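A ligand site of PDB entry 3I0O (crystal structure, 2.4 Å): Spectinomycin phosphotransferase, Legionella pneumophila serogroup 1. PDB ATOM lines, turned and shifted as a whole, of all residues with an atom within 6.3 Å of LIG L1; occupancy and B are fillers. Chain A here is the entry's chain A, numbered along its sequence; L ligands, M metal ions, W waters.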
ATOM      1  N   PHE A 109     -28.922  -9.979 -20.282  1.00  0.00           N
ATOM      2  CA  PHE A 109     -29.701  -9.669 -21.492  1.00  0.00           C
ATOM      3  C   PHE A 109     -30.486  -8.364 -21.267  1.00  0.00           C
ATOM      4  O   PHE A 109     -30.901  -7.701 -22.220  1.00  0.00           O
ATOM      5  CB  PHE A 109     -30.708 -10.800 -21.784  1.00  0.00           C
ATOM      6  CG  PHE A 109     -30.087 -12.075 -22.277  1.00  0.00           C
ATOM      7  CD1 PHE A 109     -30.711 -13.307 -22.025  1.00  0.00           C
ATOM      8  CD2 PHE A 109     -28.904 -12.069 -23.019  1.00  0.00           C
ATOM      9  CE1 PHE A 109     -30.163 -14.490 -22.495  1.00  0.00           C
ATOM     10  CE2 PHE A 109     -28.346 -13.246 -23.496  1.00  0.00           C
ATOM     11  CZ  PHE A 109     -28.978 -14.471 -23.235  1.00  0.00           C
ATOM     12  N   ASP A 212     -20.860 -22.147 -20.985  1.00  0.00           N
ATOM     13  CA  ASP A 212     -22.049 -21.461 -21.446  1.00  0.00           C
ATOM     14  C   ASP A 212     -22.207 -20.115 -20.745  1.00  0.00           C
ATOM     15  O   ASP A 212     -23.316 -19.735 -20.363  1.00  0.00           O
ATOM     16  CB  ASP A 212     -23.240 -22.382 -21.199  1.00  0.00           C
ATOM     17  CG  ASP A 212     -24.520 -21.879 -21.832  1.00  0.00           C
ATOM     18  OD1 ASP A 212     -24.500 -21.505 -23.024  1.00  0.00           O
ATOM     19  OD2 ASP A 212     -25.566 -21.899 -21.124  1.00  0.00           O
ATOM     20  N   HIS A 214     -22.649 -16.726 -21.220  1.00  0.00           N
ATOM     21  CA  HIS A 214     -23.051 -15.577 -22.002  1.00  0.00           C
ATOM     22  C   HIS A 214     -23.791 -14.673 -21.008  1.00  0.00           C
ATOM     23  O   HIS A 214     -23.886 -15.002 -19.832  1.00  0.00           O
ATOM     24  CB  HIS A 214     -23.966 -16.001 -23.145  1.00  0.00           C
ATOM     25  CG  HIS A 214     -25.094 -16.886 -22.734  1.00  0.00           C
ATOM     26  ND1 HIS A 214     -26.234 -16.409 -22.124  1.00  0.00           N
ATOM     27  CD2 HIS A 214     -25.276 -18.227 -22.866  1.00  0.00           C
ATOM     28  CE1 HIS A 214     -27.065 -17.418 -21.894  1.00  0.00           C
ATOM     29  NE2 HIS A 214     -26.511 -18.526 -22.333  1.00  0.00           N
ATOM     30  N   ASN A 217     -26.403 -15.873 -18.425  1.00  0.00           N
ATOM     31  CA  ASN A 217     -25.942 -16.616 -17.279  1.00  0.00           C
ATOM     32  C   ASN A 217     -25.117 -15.786 -16.330  1.00  0.00           C
ATOM     33  O   ASN A 217     -24.247 -16.286 -15.615  1.00  0.00           O
ATOM     34  CB  ASN A 217     -25.191 -17.876 -17.723  1.00  0.00           C
ATOM     35  CG  ASN A 217     -26.129 -18.946 -18.249  1.00  0.00           C
ATOM     36  OD1 ASN A 217     -27.219 -19.122 -17.706  1.00  0.00           O
ATOM     37  ND2 ASN A 217     -25.716 -19.653 -19.294  1.00  0.00           N
ATOM     38  N   ASP A 230     -25.949 -20.950 -13.660  1.00  0.00           N
ATOM     39  CA  ASP A 230     -26.076 -22.033 -14.629  1.00  0.00           C
ATOM     40  C   ASP A 230     -24.814 -22.882 -14.679  1.00  0.00           C
ATOM     41  O   ASP A 230     -24.116 -22.922 -15.695  1.00  0.00           O
ATOM     42  CB  ASP A 230     -26.364 -21.442 -16.021  1.00  0.00           C
ATOM     43  CG  ASP A 230     -27.333 -22.294 -16.840  1.00  0.00           C
ATOM     44  OD1 ASP A 230     -27.569 -23.466 -16.483  1.00  0.00           O
ATOM     45  OD2 ASP A 230     -27.871 -21.777 -17.844  1.00  0.00           O
ATOM     46  N   GLU A 233     -23.145 -27.338 -17.076  1.00  0.00           N
ATOM     47  CA  GLU A 233     -22.276 -27.895 -18.104  1.00  0.00           C
ATOM     48  C   GLU A 233     -20.784 -27.664 -17.893  1.00  0.00           C
ATOM     49  O   GLU A 233     -20.043 -27.551 -18.859  1.00  0.00           O
ATOM     50  CB  GLU A 233     -22.656 -27.318 -19.476  1.00  0.00           C
ATOM     51  CG  GLU A 233     -24.154 -27.315 -19.766  1.00  0.00           C
ATOM     52  CD  GLU A 233     -24.727 -28.707 -19.945  1.00  0.00           C
ATOM     53  OE1 GLU A 233     -24.455 -29.591 -19.107  1.00  0.00           O
ATOM     54  OE2 GLU A 233     -25.456 -28.921 -20.935  1.00  0.00           O
ATOM     55  N   VAL A 250     -24.037 -13.195 -27.990  1.00  0.00           N
ATOM     56  CA  VAL A 250     -25.201 -13.976 -27.614  1.00  0.00           C
ATOM     57  C   VAL A 250     -26.275 -13.069 -27.008  1.00  0.00           C
ATOM     58  O   VAL A 250     -26.003 -12.282 -26.099  1.00  0.00           O
ATOM     59  CB  VAL A 250     -24.855 -15.118 -26.592  1.00  0.00           C
ATOM     60  CG1 VAL A 250     -26.126 -15.849 -26.151  1.00  0.00           C
ATOM     61  CG2 VAL A 250     -23.891 -16.110 -27.221  1.00  0.00           C
ATOM     62  N   GLY A 251     -27.500 -13.172 -27.538  1.00  0.00           N
ATOM     63  CA  GLY A 251     -28.590 -12.352 -27.041  1.00  0.00           C
ATOM     64  C   GLY A 251     -28.548 -10.894 -27.499  1.00  0.00           C
ATOM     65  O   GLY A 251     -29.246 -10.032 -26.935  1.00  0.00           O
ATOM     66  N   ARG A 284     -20.937 -23.603 -31.553  1.00  0.00           N
ATOM     67  CA  ARG A 284     -22.029 -23.319 -30.634  1.00  0.00           C
ATOM     68  C   ARG A 284     -23.312 -22.988 -31.401  1.00  0.00           C
ATOM     69  O   ARG A 284     -24.397 -23.396 -31.001  1.00  0.00           O
ATOM     70  CB  ARG A 284     -21.669 -22.178 -29.676  1.00  0.00           C
ATOM     71  CG  ARG A 284     -22.785 -21.896 -28.683  1.00  0.00           C
ATOM     72  CD  ARG A 284     -22.416 -20.867 -27.640  1.00  0.00           C
ATOM     73  NE  ARG A 284     -23.402 -20.872 -26.570  1.00  0.00           N
ATOM     74  CZ  ARG A 284     -24.571 -20.248 -26.612  1.00  0.00           C
ATOM     75  NH1 ARG A 284     -24.915 -19.529 -27.677  1.00  0.00           N
ATOM     76  NH2 ARG A 284     -25.418 -20.352 -25.601  1.00  0.00           N
ATOM     77  N   GLU A 287     -24.771 -26.122 -32.832  1.00  0.00           N
ATOM     78  CA  GLU A 287     -25.503 -26.851 -31.798  1.00  0.00           C
ATOM     79  C   GLU A 287     -26.921 -26.293 -31.663  1.00  0.00           C
ATOM     80  O   GLU A 287     -27.899 -27.044 -31.627  1.00  0.00           O
ATOM     81  CB  GLU A 287     -24.774 -26.783 -30.447  1.00  0.00           C
ATOM     82  CG  GLU A 287     -25.382 -27.700 -29.359  1.00  0.00           C
ATOM     83  CD  GLU A 287     -24.544 -27.784 -28.070  1.00  0.00           C
ATOM     84  OE1 GLU A 287     -23.303 -27.930 -28.163  1.00  0.00           O
ATOM     85  OE2 GLU A 287     -25.127 -27.716 -26.973  1.00  0.00           O
ATOM     86  N   ASP A 288     -27.033 -24.962 -31.596  1.00  0.00           N
ATOM     87  CA  ASP A 288     -28.342 -24.366 -31.465  1.00  0.00           C
ATOM     88  C   ASP A 288     -29.204 -24.683 -32.679  1.00  0.00           C
ATOM     89  O   ASP A 288     -30.379 -24.996 -32.538  1.00  0.00           O
ATOM     90  CB  ASP A 288     -28.244 -22.851 -31.256  1.00  0.00           C
ATOM     91  CG  ASP A 288     -28.041 -22.471 -29.791  1.00  0.00           C
ATOM     92  OD1 ASP A 288     -28.124 -23.364 -28.913  1.00  0.00           O
ATOM     93  OD2 ASP A 288     -27.821 -21.283 -29.510  1.00  0.00           O
ATOM     94  N   VAL A 291     -30.418 -28.227 -32.149  1.00  0.00           N
ATOM     95  CA  VAL A 291     -31.437 -28.388 -31.118  1.00  0.00           C
ATOM     96  C   VAL A 291     -32.765 -27.768 -31.533  1.00  0.00           C
ATOM     97  O   VAL A 291     -33.817 -28.374 -31.373  1.00  0.00           O
ATOM     98  CB  VAL A 291     -30.971 -27.793 -29.769  1.00  0.00           C
ATOM     99  CG1 VAL A 291     -32.151 -27.744 -28.785  1.00  0.00           C
ATOM    100  CG2 VAL A 291     -29.829 -28.634 -29.187  1.00  0.00           C
ATOM    101  N   TYR A 292     -32.721 -26.542 -32.054  1.00  0.00           N
ATOM    102  CA  TYR A 292     -33.941 -25.875 -32.493  1.00  0.00           C
ATOM    103  C   TYR A 292     -34.506 -26.588 -33.713  1.00  0.00           C
ATOM    104  O   TYR A 292     -35.721 -26.742 -33.844  1.00  0.00           O
ATOM    105  CB  TYR A 292     -33.650 -24.405 -32.826  1.00  0.00           C
ATOM    106  CG  TYR A 292     -33.253 -23.601 -31.612  1.00  0.00           C
ATOM    107  CD1 TYR A 292     -32.357 -22.529 -31.725  1.00  0.00           C
ATOM    108  CD2 TYR A 292     -33.727 -23.934 -30.343  1.00  0.00           C
ATOM    109  CE1 TYR A 292     -31.956 -21.818 -30.607  1.00  0.00           C
ATOM    110  CE2 TYR A 292     -33.335 -23.228 -29.218  1.00  0.00           C
ATOM    111  CZ  TYR A 292     -32.445 -22.166 -29.361  1.00  0.00           C
ATOM    112  OH  TYR A 292     -32.028 -21.478 -28.254  1.00  0.00           O
ATOM    113  N   TYR A 312     -35.823 -18.084 -31.360  1.00  0.00           N
ATOM    114  CA  TYR A 312     -34.397 -18.104 -31.052  1.00  0.00           C
ATOM    115  C   TYR A 312     -33.561 -18.461 -32.267  1.00  0.00           C
ATOM    116  O   TYR A 312     -32.503 -17.891 -32.503  1.00  0.00           O
ATOM    117  CB  TYR A 312     -34.128 -19.104 -29.928  1.00  0.00           C
ATOM    118  CG  TYR A 312     -34.578 -18.603 -28.583  1.00  0.00           C
ATOM    119  CD1 TYR A 312     -34.952 -19.483 -27.581  1.00  0.00           C
ATOM    120  CD2 TYR A 312     -34.590 -17.234 -28.298  1.00  0.00           C
ATOM    121  CE1 TYR A 312     -35.325 -19.024 -26.311  1.00  0.00           C
ATOM    122  CE2 TYR A 312     -34.962 -16.760 -27.041  1.00  0.00           C
ATOM    123  CZ  TYR A 312     -35.323 -17.669 -26.057  1.00  0.00           C
ATOM    124  OH  TYR A 312     -35.690 -17.224 -24.803  1.00  0.00           O
ATOM    125  N   PHE A 313     -34.053 -19.407 -33.049  1.00  0.00           N
ATOM    126  CA  PHE A 313     -33.368 -19.816 -34.251  1.00  0.00           C
ATOM    127  C   PHE A 313     -33.126 -18.590 -35.145  1.00  0.00           C
ATOM    128  O   PHE A 313     -31.980 -18.272 -35.489  1.00  0.00           O
ATOM    129  CB  PHE A 313     -34.191 -20.864 -34.990  1.00  0.00           C
ATOM    130  CG  PHE A 313     -33.487 -21.459 -36.180  1.00  0.00           C
ATOM    131  CD1 PHE A 313     -32.754 -22.624 -36.048  1.00  0.00           C
ATOM    132  CD2 PHE A 313     -33.553 -20.854 -37.417  1.00  0.00           C
ATOM    133  CE1 PHE A 313     -32.085 -23.187 -37.139  1.00  0.00           C
ATOM    134  CE2 PHE A 313     -32.891 -21.401 -38.506  1.00  0.00           C
ATOM    135  CZ  PHE A 313     -32.158 -22.567 -38.374  1.00  0.00           C
ATOM    136  N   GLU A 315     -33.421 -15.448 -34.426  1.00  0.00           N
ATOM    137  CA  GLU A 315     -32.721 -14.416 -33.657  1.00  0.00           C
ATOM    138  C   GLU A 315     -31.215 -14.463 -33.931  1.00  0.00           C
ATOM    139  O   GLU A 315     -30.546 -13.434 -33.981  1.00  0.00           O
ATOM    140  CB  GLU A 315     -33.001 -14.642 -32.169  1.00  0.00           C
ATOM    141  CG  GLU A 315     -32.776 -13.442 -31.251  1.00  0.00           C
ATOM    142  CD  GLU A 315     -31.585 -13.634 -30.324  1.00  0.00           C
ATOM    143  OE1 GLU A 315     -31.366 -14.781 -29.850  1.00  0.00           O
ATOM    144  OE2 GLU A 315     -30.868 -12.635 -30.040  1.00  0.00           O
ATOM    145  N   MET A 316     -30.686 -15.669 -34.144  1.00  0.00           N
ATOM    146  CA  MET A 316     -29.271 -15.832 -34.396  1.00  0.00           C
ATOM    147  C   MET A 316     -28.735 -15.157 -35.664  1.00  0.00           C
ATOM    148  O   MET A 316     -27.548 -14.809 -35.744  1.00  0.00           O
ATOM    149  CB  MET A 316     -28.932 -17.320 -34.471  1.00  0.00           C
ATOM    150  CG  MET A 316     -29.442 -18.142 -33.301  1.00  0.00           C
ATOM    151  SD  MET A 316     -28.713 -19.771 -33.295  1.00  0.00           S
ATOM    152  CE  MET A 316     -29.408 -20.507 -34.750  1.00  0.00           C
ATOM    153  N   ASN A 321     -25.620 -10.195 -34.516  1.00  0.00           N
ATOM    154  CA  ASN A 321     -25.868 -11.301 -33.585  1.00  0.00           C
ATOM    155  C   ASN A 321     -24.797 -12.377 -33.812  1.00  0.00           C
ATOM    156  O   ASN A 321     -23.876 -12.199 -34.627  1.00  0.00           O
ATOM    157  CB  ASN A 321     -27.274 -11.869 -33.772  1.00  0.00           C
ATOM    158  CG  ASN A 321     -27.810 -12.544 -32.503  1.00  0.00           C
ATOM    159  OD1 ASN A 321     -27.389 -13.646 -32.139  1.00  0.00           O
ATOM    160  ND2 ASN A 321     -28.722 -11.865 -31.808  1.00  0.00           N
HETATM  161  O1  LIG L   1     -29.923 -18.626 -24.543  1.00  0.00           O
HETATM  162  C1  LIG L   1     -30.786 -17.694 -25.250  1.00  0.00           C
HETATM  163  C2  LIG L   1     -32.026 -17.446 -24.409  1.00  0.00           C
HETATM  164  C3  LIG L   1     -31.175 -18.283 -26.661  1.00  0.00           C
HETATM  165  C4  LIG L   1     -29.870 -18.512 -27.390  1.00  0.00           C
HETATM  166  C5  LIG L   1     -29.168 -19.565 -26.549  1.00  0.00           C
HETATM  167  O2  LIG L   1     -27.939 -19.842 -27.236  1.00  0.00           O
HETATM  168  C6  LIG L   1     -28.703 -18.933 -25.268  1.00  0.00           C
HETATM  169  O3  LIG L   1     -29.893 -20.780 -26.416  1.00  0.00           O
HETATM  170  O4  LIG L   1     -28.105 -19.865 -24.354  1.00  0.00           O
HETATM  171  C7  LIG L   1     -29.114 -21.693 -25.665  1.00  0.00           C
HETATM  172  C8  LIG L   1     -29.882 -23.020 -25.563  1.00  0.00           C
HETATM  173  N1  LIG L   1     -30.104 -23.483 -26.958  1.00  0.00           N
HETATM  174  C9  LIG L   1     -30.852 -24.743 -26.978  1.00  0.00           C
HETATM  175  C10 LIG L   1     -28.995 -24.038 -24.768  1.00  0.00           C
HETATM  176  O5  LIG L   1     -27.750 -24.222 -25.466  1.00  0.00           O
HETATM  177  C11 LIG L   1     -28.701 -23.468 -23.345  1.00  0.00           C
HETATM  178  N2  LIG L   1     -27.891 -24.305 -22.622  1.00  0.00           N
HETATM  179  C12 LIG L   1     -28.466 -25.644 -22.401  1.00  0.00           C
HETATM  180  C13 LIG L   1     -28.002 -22.118 -23.474  1.00  0.00           C
HETATM  181  O6  LIG L   1     -27.763 -21.611 -22.182  1.00  0.00           O
HETATM  182  C14 LIG L   1     -28.842 -21.125 -24.261  1.00  0.00           C
HETATM  183  O7  LIG L   1     -30.009 -19.005 -28.717  1.00  0.00           O
HETATM  184  O8  LIG L   1     -29.448 -17.212 -27.440  1.00  0.00           O
HETATM  185  P1  LG2 L   2     -31.417 -22.701 -16.834  1.00  0.00           P
HETATM  186  O1  LG2 L   2     -30.239 -23.571 -17.080  1.00  0.00           O
HETATM  187  O2  LG2 L   2     -32.783 -23.291 -16.883  1.00  0.00           O
HETATM  188  O3  LG2 L   2     -31.360 -21.460 -17.876  1.00  0.00           O
HETATM  189  P2  LG2 L   2     -30.186 -20.823 -15.020  1.00  0.00           P
HETATM  190  O4  LG2 L   2     -29.344 -21.302 -13.901  1.00  0.00           O
HETATM  191  O5  LG2 L   2     -29.534 -20.319 -16.247  1.00  0.00           O
HETATM  192  O6  LG2 L   2     -31.240 -22.002 -15.393  1.00  0.00           O
HETATM  193  O7  LG2 L   2     -31.168 -19.660 -14.469  1.00  0.00           O
HETATM  194  C1  LG2 L   2     -32.180 -19.083 -15.314  1.00  0.00           C
HETATM  195  C2  LG2 L   2     -32.792 -17.832 -14.688  1.00  0.00           C
HETATM  196  O8  LG2 L   2     -33.290 -18.101 -13.360  1.00  0.00           O
HETATM  197  C3  LG2 L   2     -31.815 -16.657 -14.475  1.00  0.00           C
HETATM  198  O9  LG2 L   2     -31.880 -15.768 -15.599  1.00  0.00           O
HETATM  199  C4  LG2 L   2     -32.426 -15.962 -13.244  1.00  0.00           C
HETATM  200  O10 LG2 L   2     -33.473 -15.066 -13.684  1.00  0.00           O
HETATM  201  C5  LG2 L   2     -33.050 -17.076 -12.385  1.00  0.00           C
HETATM  202  N1  LG2 L   2     -32.219 -17.480 -11.206  1.00  0.00           N
HETATM  203  C6  LG2 L   2     -31.217 -18.422 -11.132  1.00  0.00           C
HETATM  204  N2  LG2 L   2     -30.672 -18.540  -9.953  1.00  0.00           N
HETATM  205  C7  LG2 L   2     -31.347 -17.611  -9.175  1.00  0.00           C
HETATM  206  C8  LG2 L   2     -31.250 -17.218  -7.786  1.00  0.00           C
HETATM  207  N3  LG2 L   2     -30.386 -17.758  -6.947  1.00  0.00           N
HETATM  208  N4  LG2 L   2     -32.093 -16.244  -7.340  1.00  0.00           N
HETATM  209  C9  LG2 L   2     -32.976 -15.684  -8.189  1.00  0.00           C
HETATM  210  N5  LG2 L   2     -33.165 -15.960  -9.493  1.00  0.00           N
HETATM  211  C10 LG2 L   2     -32.304 -16.953  -9.929  1.00  0.00           C
HETATM  212 MG    MG M   1     -29.215 -20.101 -18.153  1.00  0.00          MG
HETATM  213  O   HOH W   1     -30.321 -18.288 -21.864  1.00  0.00           O
HETATM  214  O   HOH W   2     -30.860 -17.155 -30.344  1.00  0.00           O
HETATM  215  O   HOH W   3     -27.071 -17.371 -29.323  1.00  0.00           O
HETATM  216  O   HOH W   4     -25.056 -24.496 -23.438  1.00  0.00           O
HETATM  217  O   HOH W   5     -27.650 -26.519 -26.584  1.00  0.00           O
HETATM  218  O   HOH W   6     -25.568 -24.274 -28.164  1.00  0.00           O
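Phe 109 touches LIG L1. CG1 of Val 250 touches O8 of LIG L1, at 3.8 Å. Val 291 touches LIG L1. Tyr 312 touches LIG L1 (OH to C2, 3.7 Å). Glu 315 touches LIG L1. Hydrophobic or aromatic side chains that line LIG L1: Phe 109, His 214, Val 250, Val 291, Tyr 292 and Tyr 312. Of the 18 residues printed, 10 come within 4 Å of LIG L1. The nearest printed residue that does not touch LIG L1 is Asn 217 (4.05 Å).
OD2 of Asp 212 is in salt-bridge range of N2 of LIG L1. OD1 of Asp 288 lies within salt-bridge range of N1 of LIG L1 (2.8 Å). An oxygen (O4) of LIG L1 is in hydrogen-bond range of a ring nitrogen (NE2) of His 214. The side-chain hydroxyl (OH) of Tyr 292 is in hydrogen-bond range of an oxygen (O3) of LIG L1, 2.9 Å away. NH2 of Arg 284 is in hydrogen-bond range of O4 of LIG L1 (3.0 Å). The backbone NH (N) of Asp 230 sits at hydrogen-bond distance from an oxygen (O4) of LG2 L2.
The side-chain carboxylate (OD1) of Asp 212 lies within salt-bridge range of the guanidinium group (NH2) of Arg 284 (3.0 Å). ND2 of Asn 217 is in hydrogen-bond range of O of Asp 212 (2.6 Å). OD2 of Asp 288 is in salt-bridge range of NH1 of Arg 284. ND2 of Asn 217 lies within hydrogen-bond range of NE2 of His 214, 3.3 Å away. OE2 of Glu 315 lies within hydrogen-bond range of ND2 of Asn 321.
Water W5 lies within hydrogen-bond range of O5 of LIG L1 (2.6 Å) and OE2 of Glu 287 (2.8 Å). Water W2 lies within hydrogen-bond range of OE1 of Glu 315, O7 of LIG L1 and O of Tyr 312. Water W4 bridges N2 of LIG L1 and OD1 of Asp 212. Water W3 bridges an oxygen (O8) of LIG L1 and the guanidinium group of Arg 284. Water W6 lies within hydrogen-bond range of OD1 of Asp 288 (2.8 Å), O of Arg 284 (3.2 Å) and O5 of LIG L1 (3.5 Å).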
